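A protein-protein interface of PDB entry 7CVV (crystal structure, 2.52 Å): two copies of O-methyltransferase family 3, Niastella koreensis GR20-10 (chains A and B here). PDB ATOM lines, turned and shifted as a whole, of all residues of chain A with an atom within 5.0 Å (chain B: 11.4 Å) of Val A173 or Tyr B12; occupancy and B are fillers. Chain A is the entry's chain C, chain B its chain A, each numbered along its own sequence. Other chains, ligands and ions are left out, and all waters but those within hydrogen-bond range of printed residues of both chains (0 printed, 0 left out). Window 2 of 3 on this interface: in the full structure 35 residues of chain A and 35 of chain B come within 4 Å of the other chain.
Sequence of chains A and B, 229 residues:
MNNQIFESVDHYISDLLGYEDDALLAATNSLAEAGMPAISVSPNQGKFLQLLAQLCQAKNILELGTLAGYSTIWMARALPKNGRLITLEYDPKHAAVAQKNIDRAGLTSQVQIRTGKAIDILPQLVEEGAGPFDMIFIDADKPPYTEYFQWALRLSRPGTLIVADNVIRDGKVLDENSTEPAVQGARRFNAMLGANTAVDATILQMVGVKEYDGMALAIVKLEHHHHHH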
ATOM      1  N   VAL A 167      24.289  17.175  26.535  1.00  0.00           N
ATOM      2  CA  VAL A 167      23.561  16.320  25.560  1.00  0.00           C
ATOM      3  C   VAL A 167      23.543  14.868  26.056  1.00  0.00           C
ATOM      4  O   VAL A 167      23.065  14.006  25.286  1.00  0.00           O
ATOM      5  CB  VAL A 167      24.167  16.442  24.144  1.00  0.00           C
ATOM      6  CG1 VAL A 167      24.298  17.899  23.735  1.00  0.00           C
ATOM      7  CG2 VAL A 167      25.506  15.736  23.991  1.00  0.00           C
ATOM      8  N   ILE A 168      24.044  14.605  27.270  1.00  0.00           N
ATOM      9  CA  ILE A 168      24.145  13.244  27.892  1.00  0.00           C
ATOM     10  C   ILE A 168      23.220  13.145  29.117  1.00  0.00           C
ATOM     11  O   ILE A 168      22.707  12.054  29.353  1.00  0.00           O
ATOM     12  CB  ILE A 168      25.624  12.933  28.202  1.00  0.00           C
ATOM     13  CG1 ILE A 168      26.379  12.641  26.909  1.00  0.00           C
ATOM     14  CG2 ILE A 168      25.799  11.793  29.188  1.00  0.00           C
ATOM     15  CD1 ILE A 168      25.774  11.512  26.104  1.00  0.00           C
ATOM     16  N   ARG A 169      23.027  14.232  29.866  1.00  0.00           N
ATOM     17  CA  ARG A 169      22.057  14.321  30.990  1.00  0.00           C
ATOM     18  C   ARG A 169      22.356  13.270  32.056  1.00  0.00           C
ATOM     19  O   ARG A 169      21.432  12.512  32.378  1.00  0.00           O
ATOM     20  CB  ARG A 169      20.627  14.062  30.508  1.00  0.00           C
ATOM     21  CG  ARG A 169      20.262  14.745  29.202  1.00  0.00           C
ATOM     22  CD  ARG A 169      20.358  16.246  29.327  1.00  0.00           C
ATOM     23  NE  ARG A 169      19.457  16.736  30.356  1.00  0.00           N
ATOM     24  CZ  ARG A 169      19.680  17.817  31.096  1.00  0.00           C
ATOM     25  NH1 ARG A 169      18.789  18.185  32.002  1.00  0.00           N
ATOM     26  NH2 ARG A 169      20.782  18.526  30.928  1.00  0.00           N
ATOM     27  N   GLY A 171      23.584  10.512  31.774  1.00  0.00           N
ATOM     28  CA  GLY A 171      23.552   9.153  31.202  1.00  0.00           C
ATOM     29  C   GLY A 171      22.137   8.642  30.988  1.00  0.00           C
ATOM     30  O   GLY A 171      22.001   7.493  30.555  1.00  0.00           O
ATOM     31  N   LYS A 172      21.136   9.491  31.236  1.00  0.00           N
ATOM     32  CA  LYS A 172      19.688   9.196  31.056  1.00  0.00           C
ATOM     33  C   LYS A 172      19.306   9.097  29.571  1.00  0.00           C
ATOM     34  O   LYS A 172      18.214   8.564  29.277  1.00  0.00           O
ATOM     35  CB  LYS A 172      18.864  10.301  31.713  1.00  0.00           C
ATOM     36  CG  LYS A 172      19.053  10.414  33.215  1.00  0.00           C
ATOM     37  CD  LYS A 172      18.800  11.804  33.735  1.00  0.00           C
ATOM     38  CE  LYS A 172      17.401  11.991  34.253  1.00  0.00           C
ATOM     39  NZ  LYS A 172      17.445  12.385  35.677  1.00  0.00           N
ATOM     40  N   VAL A 173      20.146   9.594  28.662  1.00  0.00           N
ATOM     41  CA  VAL A 173      19.954   9.447  27.188  1.00  0.00           C
ATOM     42  C   VAL A 173      20.006   7.954  26.809  1.00  0.00           C
ATOM     43  O   VAL A 173      19.650   7.632  25.661  1.00  0.00           O
ATOM     44  CB  VAL A 173      20.978  10.285  26.397  1.00  0.00           C
ATOM     45  CG1 VAL A 173      20.775  11.778  26.601  1.00  0.00           C
ATOM     46  CG2 VAL A 173      22.417   9.904  26.704  1.00  0.00           C
ATOM     47  N   LEU A 174      20.417   7.064  27.724  1.00  0.00           N
ATOM     48  CA  LEU A 174      20.414   5.597  27.471  1.00  0.00           C
ATOM     49  C   LEU A 174      19.016   5.054  27.734  1.00  0.00           C
ATOM     50  O   LEU A 174      18.810   3.882  27.432  1.00  0.00           O
ATOM     51  CB  LEU A 174      21.420   4.870  28.367  1.00  0.00           C
ATOM     52  CG  LEU A 174      22.863   5.332  28.242  1.00  0.00           C
ATOM     53  CD1 LEU A 174      23.697   4.827  29.413  1.00  0.00           C
ATOM     54  CD2 LEU A 174      23.439   4.893  26.908  1.00  0.00           C
ATOM     55  N   ASP A 175      18.132   5.866  28.317  1.00  0.00           N
ATOM     56  CA  ASP A 175      16.717   5.518  28.617  1.00  0.00           C
ATOM     57  C   ASP A 175      15.812   5.992  27.466  1.00  0.00           C
ATOM     58  O   ASP A 175      15.342   7.144  27.513  1.00  0.00           O
ATOM     59  CB  ASP A 175      16.295   6.116  29.964  1.00  0.00           C
ATOM     60  CG  ASP A 175      14.944   5.644  30.477  1.00  0.00           C
ATOM     61  OD1 ASP A 175      14.478   4.571  30.013  1.00  0.00           O
ATOM     62  OD2 ASP A 175      14.371   6.350  31.352  1.00  0.00           O
ATOM     63  N   GLU A 176      15.532   5.122  26.491  1.00  0.00           N
ATOM     64  CA  GLU A 176      14.597   5.424  25.373  1.00  0.00           C
ATOM     65  C   GLU A 176      13.161   5.567  25.894  1.00  0.00           C
ATOM     66  O   GLU A 176      12.376   6.228  25.204  1.00  0.00           O
ATOM     67  CB  GLU A 176      14.673   4.361  24.279  1.00  0.00           C
ATOM     68  CG  GLU A 176      14.257   2.974  24.726  1.00  0.00           C
ATOM     69  CD  GLU A 176      14.760   1.890  23.787  1.00  0.00           C
ATOM     70  OE1 GLU A 176      13.917   1.220  23.151  1.00  0.00           O
ATOM     71  OE2 GLU A 176      15.994   1.746  23.662  1.00  0.00           O
ATOM     72  N   VAL A 183      15.634  15.001  28.327  1.00  0.00           N
ATOM     73  CA  VAL A 183      16.248  13.701  27.934  1.00  0.00           C
ATOM     74  C   VAL A 183      15.833  13.408  26.488  1.00  0.00           C
ATOM     75  O   VAL A 183      16.739  13.164  25.669  1.00  0.00           O
ATOM     76  CB  VAL A 183      15.872  12.566  28.904  1.00  0.00           C
ATOM     77  CG1 VAL A 183      16.403  11.226  28.438  1.00  0.00           C
ATOM     78  CG2 VAL A 183      16.369  12.856  30.305  1.00  0.00           C
ATOM     79  N   ALA A 186      17.559  15.742  24.086  1.00  0.00           N
ATOM     80  CA  ALA A 186      19.000  15.436  23.932  1.00  0.00           C
ATOM     81  C   ALA A 186      19.144  14.173  23.079  1.00  0.00           C
ATOM     82  O   ALA A 186      20.055  14.127  22.261  1.00  0.00           O
ATOM     83  CB  ALA A 186      19.667  15.296  25.286  1.00  0.00           C
ATOM     84  N   ARG A 187      18.269  13.187  23.244  1.00  0.00           N
ATOM     85  CA  ARG A 187      18.360  11.943  22.455  1.00  0.00           C
ATOM     86  C   ARG A 187      18.164  12.288  20.983  1.00  0.00           C
ATOM     87  O   ARG A 187      18.917  11.751  20.164  1.00  0.00           O
ATOM     88  CB  ARG A 187      17.282  10.929  22.815  1.00  0.00           C
ATOM     89  CG  ARG A 187      17.394  10.327  24.199  1.00  0.00           C
ATOM     90  CD  ARG A 187      16.347   9.243  24.337  1.00  0.00           C
ATOM     91  NE  ARG A 187      17.124   8.030  24.269  1.00  0.00           N
ATOM     92  CZ  ARG A 187      17.112   7.139  23.300  1.00  0.00           C
ATOM     93  NH1 ARG A 187      16.265   7.235  22.293  1.00  0.00           N
ATOM     94  NH2 ARG A 187      17.941   6.115  23.384  1.00  0.00           N
ATOM     95  N   ASN A 190      21.019  13.983  19.476  1.00  0.00           N
ATOM     96  CA  ASN A 190      22.193  13.076  19.365  1.00  0.00           C
ATOM     97  C   ASN A 190      22.024  12.206  18.109  1.00  0.00           C
ATOM     98  O   ASN A 190      23.015  12.072  17.347  1.00  0.00           O
ATOM     99  CB  ASN A 190      22.419  12.284  20.660  1.00  0.00           C
ATOM    100  CG  ASN A 190      22.940  13.139  21.802  1.00  0.00           C
ATOM    101  OD1 ASN A 190      23.493  14.210  21.575  1.00  0.00           O
ATOM    102  ND2 ASN A 190      22.777  12.677  23.033  1.00  0.00           N
ATOM    103  N   GLN B   4      29.511   1.293  34.806  1.00  0.00           N
ATOM    104  CA  GLN B   4      28.842   0.788  33.585  1.00  0.00           C
ATOM    105  C   GLN B   4      28.354   1.987  32.766  1.00  0.00           C
ATOM    106  O   GLN B   4      28.346   1.910  31.536  1.00  0.00           O
ATOM    107  CB  GLN B   4      27.704  -0.167  33.968  1.00  0.00           C
ATOM    108  CG  GLN B   4      27.247  -1.069  32.830  1.00  0.00           C
ATOM    109  CD  GLN B   4      28.414  -1.661  32.071  1.00  0.00           C
ATOM    110  OE1 GLN B   4      29.315  -2.270  32.653  1.00  0.00           O
ATOM    111  NE2 GLN B   4      28.431  -1.453  30.761  1.00  0.00           N
ATOM    112  N   ILE B   5      27.981   3.068  33.439  1.00  0.00           N
ATOM    113  CA  ILE B   5      27.366   4.263  32.804  1.00  0.00           C
ATOM    114  C   ILE B   5      28.370   4.915  31.842  1.00  0.00           C
ATOM    115  O   ILE B   5      27.969   5.234  30.710  1.00  0.00           O
ATOM    116  CB  ILE B   5      26.842   5.211  33.892  1.00  0.00           C
ATOM    117  CG1 ILE B   5      26.251   6.485  33.297  1.00  0.00           C
ATOM    118  CG2 ILE B   5      27.926   5.519  34.918  1.00  0.00           C
ATOM    119  CD1 ILE B   5      25.724   7.433  34.353  1.00  0.00           C
ATOM    120  N   PHE B   6      29.634   5.095  32.234  1.00  0.00           N
ATOM    121  CA  PHE B   6      30.667   5.685  31.343  1.00  0.00           C
ATOM    122  C   PHE B   6      30.832   4.790  30.120  1.00  0.00           C
ATOM    123  O   PHE B   6      31.011   5.289  28.984  1.00  0.00           O
ATOM    124  CB  PHE B   6      32.039   5.797  32.013  1.00  0.00           C
ATOM    125  CG  PHE B   6      32.067   6.691  33.219  1.00  0.00           C
ATOM    126  CD1 PHE B   6      31.393   7.899  33.209  1.00  0.00           C
ATOM    127  CD2 PHE B   6      32.748   6.312  34.362  1.00  0.00           C
ATOM    128  CE1 PHE B   6      31.406   8.722  34.320  1.00  0.00           C
ATOM    129  CE2 PHE B   6      32.748   7.136  35.476  1.00  0.00           C
ATOM    130  CZ  PHE B   6      32.085   8.339  35.449  1.00  0.00           C
ATOM    131  N   GLU B   7      30.826   3.487  30.373  1.00  0.00           N
ATOM    132  CA  GLU B   7      31.136   2.481  29.343  1.00  0.00           C
ATOM    133  C   GLU B   7      29.935   2.389  28.393  1.00  0.00           C
ATOM    134  O   GLU B   7      30.149   2.344  27.180  1.00  0.00           O
ATOM    135  CB  GLU B   7      31.585   1.194  30.041  1.00  0.00           C
ATOM    136  CG  GLU B   7      32.973   1.352  30.659  1.00  0.00           C
ATOM    137  CD  GLU B   7      33.479   0.211  31.531  1.00  0.00           C
ATOM    138  OE1 GLU B   7      34.534  -0.377  31.195  1.00  0.00           O
ATOM    139  OE2 GLU B   7      32.831  -0.076  32.558  1.00  0.00           O
ATOM    140  N   SER B   8      28.714   2.420  28.917  1.00  0.00           N
ATOM    141  CA  SER B   8      27.478   2.343  28.108  1.00  0.00           C
ATOM    142  C   SER B   8      27.349   3.604  27.259  1.00  0.00           C
ATOM    143  O   SER B   8      26.923   3.483  26.098  1.00  0.00           O
ATOM    144  CB  SER B   8      26.271   2.157  28.965  1.00  0.00           C
ATOM    145  OG  SER B   8      26.204   0.821  29.429  1.00  0.00           O
ATOM    146  N   VAL B   9      27.667   4.770  27.829  1.00  0.00           N
ATOM    147  CA  VAL B   9      27.543   6.090  27.140  1.00  0.00           C
ATOM    148  C   VAL B   9      28.565   6.161  25.993  1.00  0.00           C
ATOM    149  O   VAL B   9      28.229   6.758  24.961  1.00  0.00           O
ATOM    150  CB  VAL B   9      27.673   7.279  28.119  1.00  0.00           C
ATOM    151  CG1 VAL B   9      27.900   8.574  27.363  1.00  0.00           C
ATOM    152  CG2 VAL B   9      26.445   7.421  29.017  1.00  0.00           C
ATOM    153  N   ASP B  10      29.750   5.561  26.164  1.00  0.00           N
ATOM    154  CA  ASP B  10      30.829   5.485  25.141  1.00  0.00           C
ATOM    155  C   ASP B  10      30.347   4.639  23.957  1.00  0.00           C
ATOM    156  O   ASP B  10      30.570   5.081  22.831  1.00  0.00           O
ATOM    157  CB  ASP B  10      32.127   4.917  25.729  1.00  0.00           C
ATOM    158  CG  ASP B  10      33.408   5.435  25.088  1.00  0.00           C
ATOM    159  OD1 ASP B  10      33.458   6.636  24.714  1.00  0.00           O
ATOM    160  OD2 ASP B  10      34.366   4.646  25.000  1.00  0.00           O
ATOM    161  N   HIS B  11      29.724   3.481  24.205  1.00  0.00           N
ATOM    162  CA  HIS B  11      29.087   2.605  23.178  1.00  0.00           C
ATOM    163  C   HIS B  11      27.999   3.401  22.424  1.00  0.00           C
ATOM    164  O   HIS B  11      27.950   3.351  21.156  1.00  0.00           O
ATOM    165  CB  HIS B  11      28.579   1.287  23.819  1.00  0.00           C
ATOM    166  CG  HIS B  11      29.631   0.235  24.029  1.00  0.00           C
ATOM    167  ND1 HIS B  11      30.396  -0.290  22.984  1.00  0.00           N
ATOM    168  CD2 HIS B  11      30.039  -0.417  25.149  1.00  0.00           C
ATOM    169  CE1 HIS B  11      31.236  -1.195  23.460  1.00  0.00           C
ATOM    170  NE2 HIS B  11      31.042  -1.286  24.784  1.00  0.00           N
ATOM    171  N   TYR B  12      27.210   4.188  23.150  1.00  0.00           N
ATOM    172  CA  TYR B  12      26.125   5.025  22.575  1.00  0.00           C
ATOM    173  C   TYR B  12      26.722   6.090  21.631  1.00  0.00           C
ATOM    174  O   TYR B  12      26.200   6.276  20.489  1.00  0.00           O
ATOM    175  CB  TYR B  12      25.277   5.570  23.723  1.00  0.00           C
ATOM    176  CG  TYR B  12      24.262   6.624  23.364  1.00  0.00           C
ATOM    177  CD1 TYR B  12      24.610   7.961  23.389  1.00  0.00           C
ATOM    178  CD2 TYR B  12      22.951   6.295  23.039  1.00  0.00           C
ATOM    179  CE1 TYR B  12      23.683   8.938  23.073  1.00  0.00           C
ATOM    180  CE2 TYR B  12      22.008   7.266  22.733  1.00  0.00           C
ATOM    181  CZ  TYR B  12      22.378   8.597  22.753  1.00  0.00           C
ATOM    182  OH  TYR B  12      21.486   9.599  22.482  1.00  0.00           O
ATOM    183  N   ILE B  13      27.810   6.747  22.047  1.00  0.00           N
ATOM    184  CA  ILE B  13      28.459   7.827  21.245  1.00  0.00           C
ATOM    185  C   ILE B  13      29.086   7.210  19.993  1.00  0.00           C
ATOM    186  O   ILE B  13      28.932   7.789  18.907  1.00  0.00           O
ATOM    187  CB  ILE B  13      29.481   8.627  22.071  1.00  0.00           C
ATOM    188  CG1 ILE B  13      28.778   9.382  23.202  1.00  0.00           C
ATOM    189  CG2 ILE B  13      30.255   9.563  21.171  1.00  0.00           C
ATOM    190  CD1 ILE B  13      29.694   9.944  24.265  1.00  0.00           C
ATOM    191  N   SER B  14      29.758   6.079  20.107  1.00  0.00           N
ATOM    192  CA  SER B  14      30.483   5.489  18.948  1.00  0.00           C
ATOM    193  C   SER B  14      29.497   4.847  17.952  1.00  0.00           C
ATOM    194  O   SER B  14      29.823   4.845  16.743  1.00  0.00           O
ATOM    195  CB  SER B  14      31.574   4.556  19.391  1.00  0.00           C
ATOM    196  OG  SER B  14      31.035   3.572  20.229  1.00  0.00           O
ATOM    197  N   ASP B  15      28.314   4.398  18.398  1.00  0.00           N
ATOM    198  CA  ASP B  15      27.238   3.919  17.477  1.00  0.00           C
ATOM    199  C   ASP B  15      26.788   5.069  16.572  1.00  0.00           C
ATOM    200  O   ASP B  15      26.421   4.787  15.440  1.00  0.00           O
ATOM    201  CB  ASP B  15      25.987   3.391  18.191  1.00  0.00           C
ATOM    202  CG  ASP B  15      26.164   2.080  18.951  1.00  0.00           C
ATOM    203  OD1 ASP B  15      27.236   1.446  18.807  1.00  0.00           O
ATOM    204  OD2 ASP B  15      25.223   1.710  19.704  1.00  0.00           O
ATOM    205  N   LEU B  16      26.779   6.311  17.074  1.00  0.00           N
ATOM    206  CA  LEU B  16      26.270   7.496  16.335  1.00  0.00           C
ATOM    207  C   LEU B  16      27.392   8.201  15.571  1.00  0.00           C
ATOM    208  O   LEU B  16      27.092   8.830  14.576  1.00  0.00           O
ATOM    209  CB  LEU B  16      25.621   8.459  17.333  1.00  0.00           C
ATOM    210  CG  LEU B  16      24.422   7.913  18.099  1.00  0.00           C
ATOM    211  CD1 LEU B  16      23.906   8.945  19.088  1.00  0.00           C
ATOM    212  CD2 LEU B  16      23.310   7.503  17.155  1.00  0.00           C
ATOM    213  N   LEU B  17      28.626   8.174  16.058  1.00  0.00           N
ATOM    214  CA  LEU B  17      29.642   9.190  15.691  1.00  0.00           C
ATOM    215  C   LEU B  17      31.059   8.621  15.774  1.00  0.00           C
ATOM    216  O   LEU B  17      32.013   9.411  15.617  1.00  0.00           O
ATOM    217  CB  LEU B  17      29.466  10.349  16.672  1.00  0.00           C
ATOM    218  CG  LEU B  17      28.189  11.171  16.516  1.00  0.00           C
ATOM    219  CD1 LEU B  17      28.021  12.140  17.672  1.00  0.00           C
ATOM    220  CD2 LEU B  17      28.203  11.921  15.196  1.00  0.00           C
ATOM    221  N   GLY B  18      31.210   7.318  16.005  1.00  0.00           N
ATOM    222  CA  GLY B  18      32.534   6.676  16.156  1.00  0.00           C
ATOM    223  C   GLY B  18      32.652   5.439  15.286  1.00  0.00           C
ATOM    224  O   GLY B  18      33.342   4.497  15.681  1.00  0.00           O
ATOM    225  N   TYR B  19      31.991   5.443  14.133  1.00  0.00           N
ATOM    226  CA  TYR B  19      32.048   4.318  13.178  1.00  0.00           C
ATOM    227  C   TYR B  19      33.520   4.044  12.863  1.00  0.00           C
ATOM    228  O   TYR B  19      34.273   4.966  12.487  1.00  0.00           O
ATOM    229  CB  TYR B  19      31.216   4.595  11.928  1.00  0.00           C
ATOM    230  CG  TYR B  19      31.512   3.633  10.814  1.00  0.00           C
ATOM    231  CD1 TYR B  19      31.071   2.322  10.874  1.00  0.00           C
ATOM    232  CD2 TYR B  19      32.263   4.022   9.715  1.00  0.00           C
ATOM    233  CE1 TYR B  19      31.341   1.424   9.854  1.00  0.00           C
ATOM    234  CE2 TYR B  19      32.562   3.127   8.701  1.00  0.00           C
ATOM    235  CZ  TYR B  19      32.096   1.827   8.766  1.00  0.00           C
ATOM    236  OH  TYR B  19      32.378   0.958   7.749  1.00  0.00           O
ATOM    237  N   GLU B  20      33.889   2.780  13.029  1.00  0.00           N
ATOM    238  CA  GLU B  20      35.195   2.201  12.662  1.00  0.00           C
ATOM    239  C   GLU B  20      35.045   1.400  11.367  1.00  0.00           C
ATOM    240  O   GLU B  20      34.317   0.402  11.356  1.00  0.00           O
ATOM    241  CB  GLU B  20      35.662   1.283  13.788  1.00  0.00           C
ATOM    242  CG  GLU B  20      36.110   2.020  15.028  1.00  0.00           C
ATOM    243  CD  GLU B  20      36.811   1.058  15.957  1.00  0.00           C
ATOM    244  OE1 GLU B  20      36.175   0.048  16.299  1.00  0.00           O
ATOM    245  OE2 GLU B  20      38.002   1.279  16.262  1.00  0.00           O
ATOM    246  N   SER B  42      40.870   5.222  21.692  1.00  0.00           N
ATOM    247  CA  SER B  42      39.539   4.612  21.433  1.00  0.00           C
ATOM    248  C   SER B  42      39.010   5.197  20.127  1.00  0.00           C
ATOM    249  O   SER B  42      39.508   6.238  19.698  1.00  0.00           O
ATOM    250  CB  SER B  42      38.606   4.917  22.560  1.00  0.00           C
ATOM    251  OG  SER B  42      38.154   6.252  22.428  1.00  0.00           O
ATOM    252  N   PRO B  43      38.001   4.579  19.461  1.00  0.00           N
ATOM    253  CA  PRO B  43      37.338   5.230  18.333  1.00  0.00           C
ATOM    254  C   PRO B  43      36.908   6.683  18.640  1.00  0.00           C
ATOM    255  O   PRO B  43      37.144   7.537  17.797  1.00  0.00           O
ATOM    256  CB  PRO B  43      36.124   4.355  17.991  1.00  0.00           C
ATOM    257  CG  PRO B  43      36.158   3.203  18.979  1.00  0.00           C
ATOM    258  CD  PRO B  43      37.475   3.243  19.728  1.00  0.00           C
ATOM    259  N   ASN B  44      36.291   6.959  19.795  1.00  0.00           N
ATOM    260  CA  ASN B  44      35.708   8.300  20.076  1.00  0.00           C
ATOM    261  C   ASN B  44      36.837   9.324  20.229  1.00  0.00           C
ATOM    262  O   ASN B  44      36.696  10.437  19.728  1.00  0.00           O
ATOM    263  CB  ASN B  44      34.749   8.278  21.268  1.00  0.00           C
ATOM    264  CG  ASN B  44      33.419   7.590  20.990  1.00  0.00           C
ATOM    265  OD1 ASN B  44      32.976   7.489  19.835  1.00  0.00           O
ATOM    266  ND2 ASN B  44      32.760   7.116  22.044  1.00  0.00           N
ATOM    267  N   LYS B  47      38.033  10.011  16.746  1.00  0.00           N
ATOM    268  CA  LYS B  47      37.168  10.964  16.038  1.00  0.00           C
ATOM    269  C   LYS B  47      37.467  12.361  16.567  1.00  0.00           C
ATOM    270  O   LYS B  47      37.476  13.314  15.782  1.00  0.00           O
ATOM    271  CB  LYS B  47      35.705  10.600  16.250  1.00  0.00           C
ATOM    272  CG  LYS B  47      34.753  11.527  15.526  1.00  0.00           C
ATOM    273  CD  LYS B  47      34.980  11.534  14.038  1.00  0.00           C
ATOM    274  CE  LYS B  47      33.820  12.158  13.288  1.00  0.00           C
ATOM    275  NZ  LYS B  47      32.598  11.313  13.344  1.00  0.00           N
ATOM    276  N   VAL B 207      36.533   9.860  30.013  1.00  0.00           N
ATOM    277  CA  VAL B 207      36.023   8.546  30.501  1.00  0.00           C
ATOM    278  C   VAL B 207      35.308   7.833  29.363  1.00  0.00           C
ATOM    279  O   VAL B 207      34.902   8.483  28.388  1.00  0.00           O
ATOM    280  CB  VAL B 207      35.113   8.741  31.712  1.00  0.00           C
ATOM    281  CG1 VAL B 207      35.881   9.376  32.850  1.00  0.00           C
ATOM    282  CG2 VAL B 207      33.898   9.565  31.372  1.00  0.00           C
ATOM    283  N   GLY B 208      35.179   6.526  29.496  1.00  0.00           N
ATOM    284  CA  GLY B 208      34.720   5.628  28.429  1.00  0.00           C
ATOM    285  C   GLY B 208      35.150   4.218  28.750  1.00  0.00           C
ATOM    286  O   GLY B 208      35.253   3.890  29.938  1.00  0.00           O
ATOM    287  N   VAL B 209      35.386   3.413  27.717  1.00  0.00           N
ATOM    288  CA  VAL B 209      35.782   1.980  27.828  1.00  0.00           C
ATOM    289  C   VAL B 209      37.265   1.941  28.232  1.00  0.00           C
ATOM    290  O   VAL B 209      37.609   1.193  29.153  1.00  0.00           O
ATOM    291  CB  VAL B 209      35.444   1.217  26.525  1.00  0.00           C
ATOM    292  CG1 VAL B 209      36.217   1.735  25.308  1.00  0.00           C
ATOM    293  CG2 VAL B 209      35.626  -0.281  26.687  1.00  0.00           C
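The side-chain amide nitrogen (ND2) of Asn A190 sits close to the side-chain hydroxyl (OH) of Tyr B12, at 3.4 Å.
Printed residues of chain B within 4 Å of Ile A168: Val B9. Arg A169 touches none of the printed residues of chain B. Of chain B, only Tyr B12 comes within 4 Å of Val A173. Of the printed residues of chain B, Leu A174 touches Ser B8, Val B9 and Tyr B12. No residue of chain B comes within 4 Å of Asp A175. No residue of chain B comes within 4 Å of Val A183. No residue of chain B comes within 4 Å of Ala A186. Asn A190 touches just these residues of chain B: Tyr B12 (3.4 Å) and Leu B16 (3.7 Å). Of the printed residues of chain A, Ser B8 touches Leu A174 (3.7 Å). Of the printed residues of chain A, Val B9 touches Ile A168 and Leu A174. Of chain A, only Val A173 (3.8 Å), Leu A174 (3.7 Å), Arg A187 (3.9 Å) and Asn A190 (3.4 Å) come within 4 Å of Tyr B12. Of the printed residues of chain A, Leu B16 touches Asn A190. Asn B44 touches none of the printed residues of chain A. The nearest residue of chain A that does not touch Tyr B12 is Ile A168 (4.5 Å). The nearest printed residue of chain A that does not touch Ser B8 is Gly A171 (7.0 Å).
Of the 24 printed residues of chain B, 4 touch a printed residue of chain A. Printed residues of chain B that touch a printed residue of chain A: Ser B8, Val B9, Tyr B12 and Leu B16. Hydrophobic or aromatic side chains of chain B that line the printed part of chain A: Val B9, Tyr B12 and Leu B16. Hydrophobic or aromatic side chains of chain A within 4 Å of the printed part of chain B: Ile A168, Val A173 and Leu A174. Along chain A the printed residues that touch a printed residue of chain B span positions 168 to 190.
Among the printed residues, merely in contact across the chains: Asn A190 with Leu B16, Leu A174 with Ser B8, Leu A174 with Tyr B12, Val A173 with Tyr B12, Leu A174 with Val B9, Ile A168 with Val B9 and Arg A187 with Tyr B12.
No position is printed for both chains. Of the 8 pairs that touch across the chains among the printed residues, none has its exchanged pair printed and touching as well.
O of Val A167 is in hydrogen-bond range of ND2 of Asn A190, 2.6 Å away. O of Val A173 is in hydrogen-bond range of NE of Arg A187 (2.9 Å). The side-chain amide nitrogen (ND2) of Asn A190 sits close to the backbone carbonyl oxygen (O) of Ala A186, at 3.2 Å. The backbone carbonyl oxygen of Gln B4 sits at hydrogen-bond distance from the side-chain hydroxyl of Ser B8 (3.2 Å).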
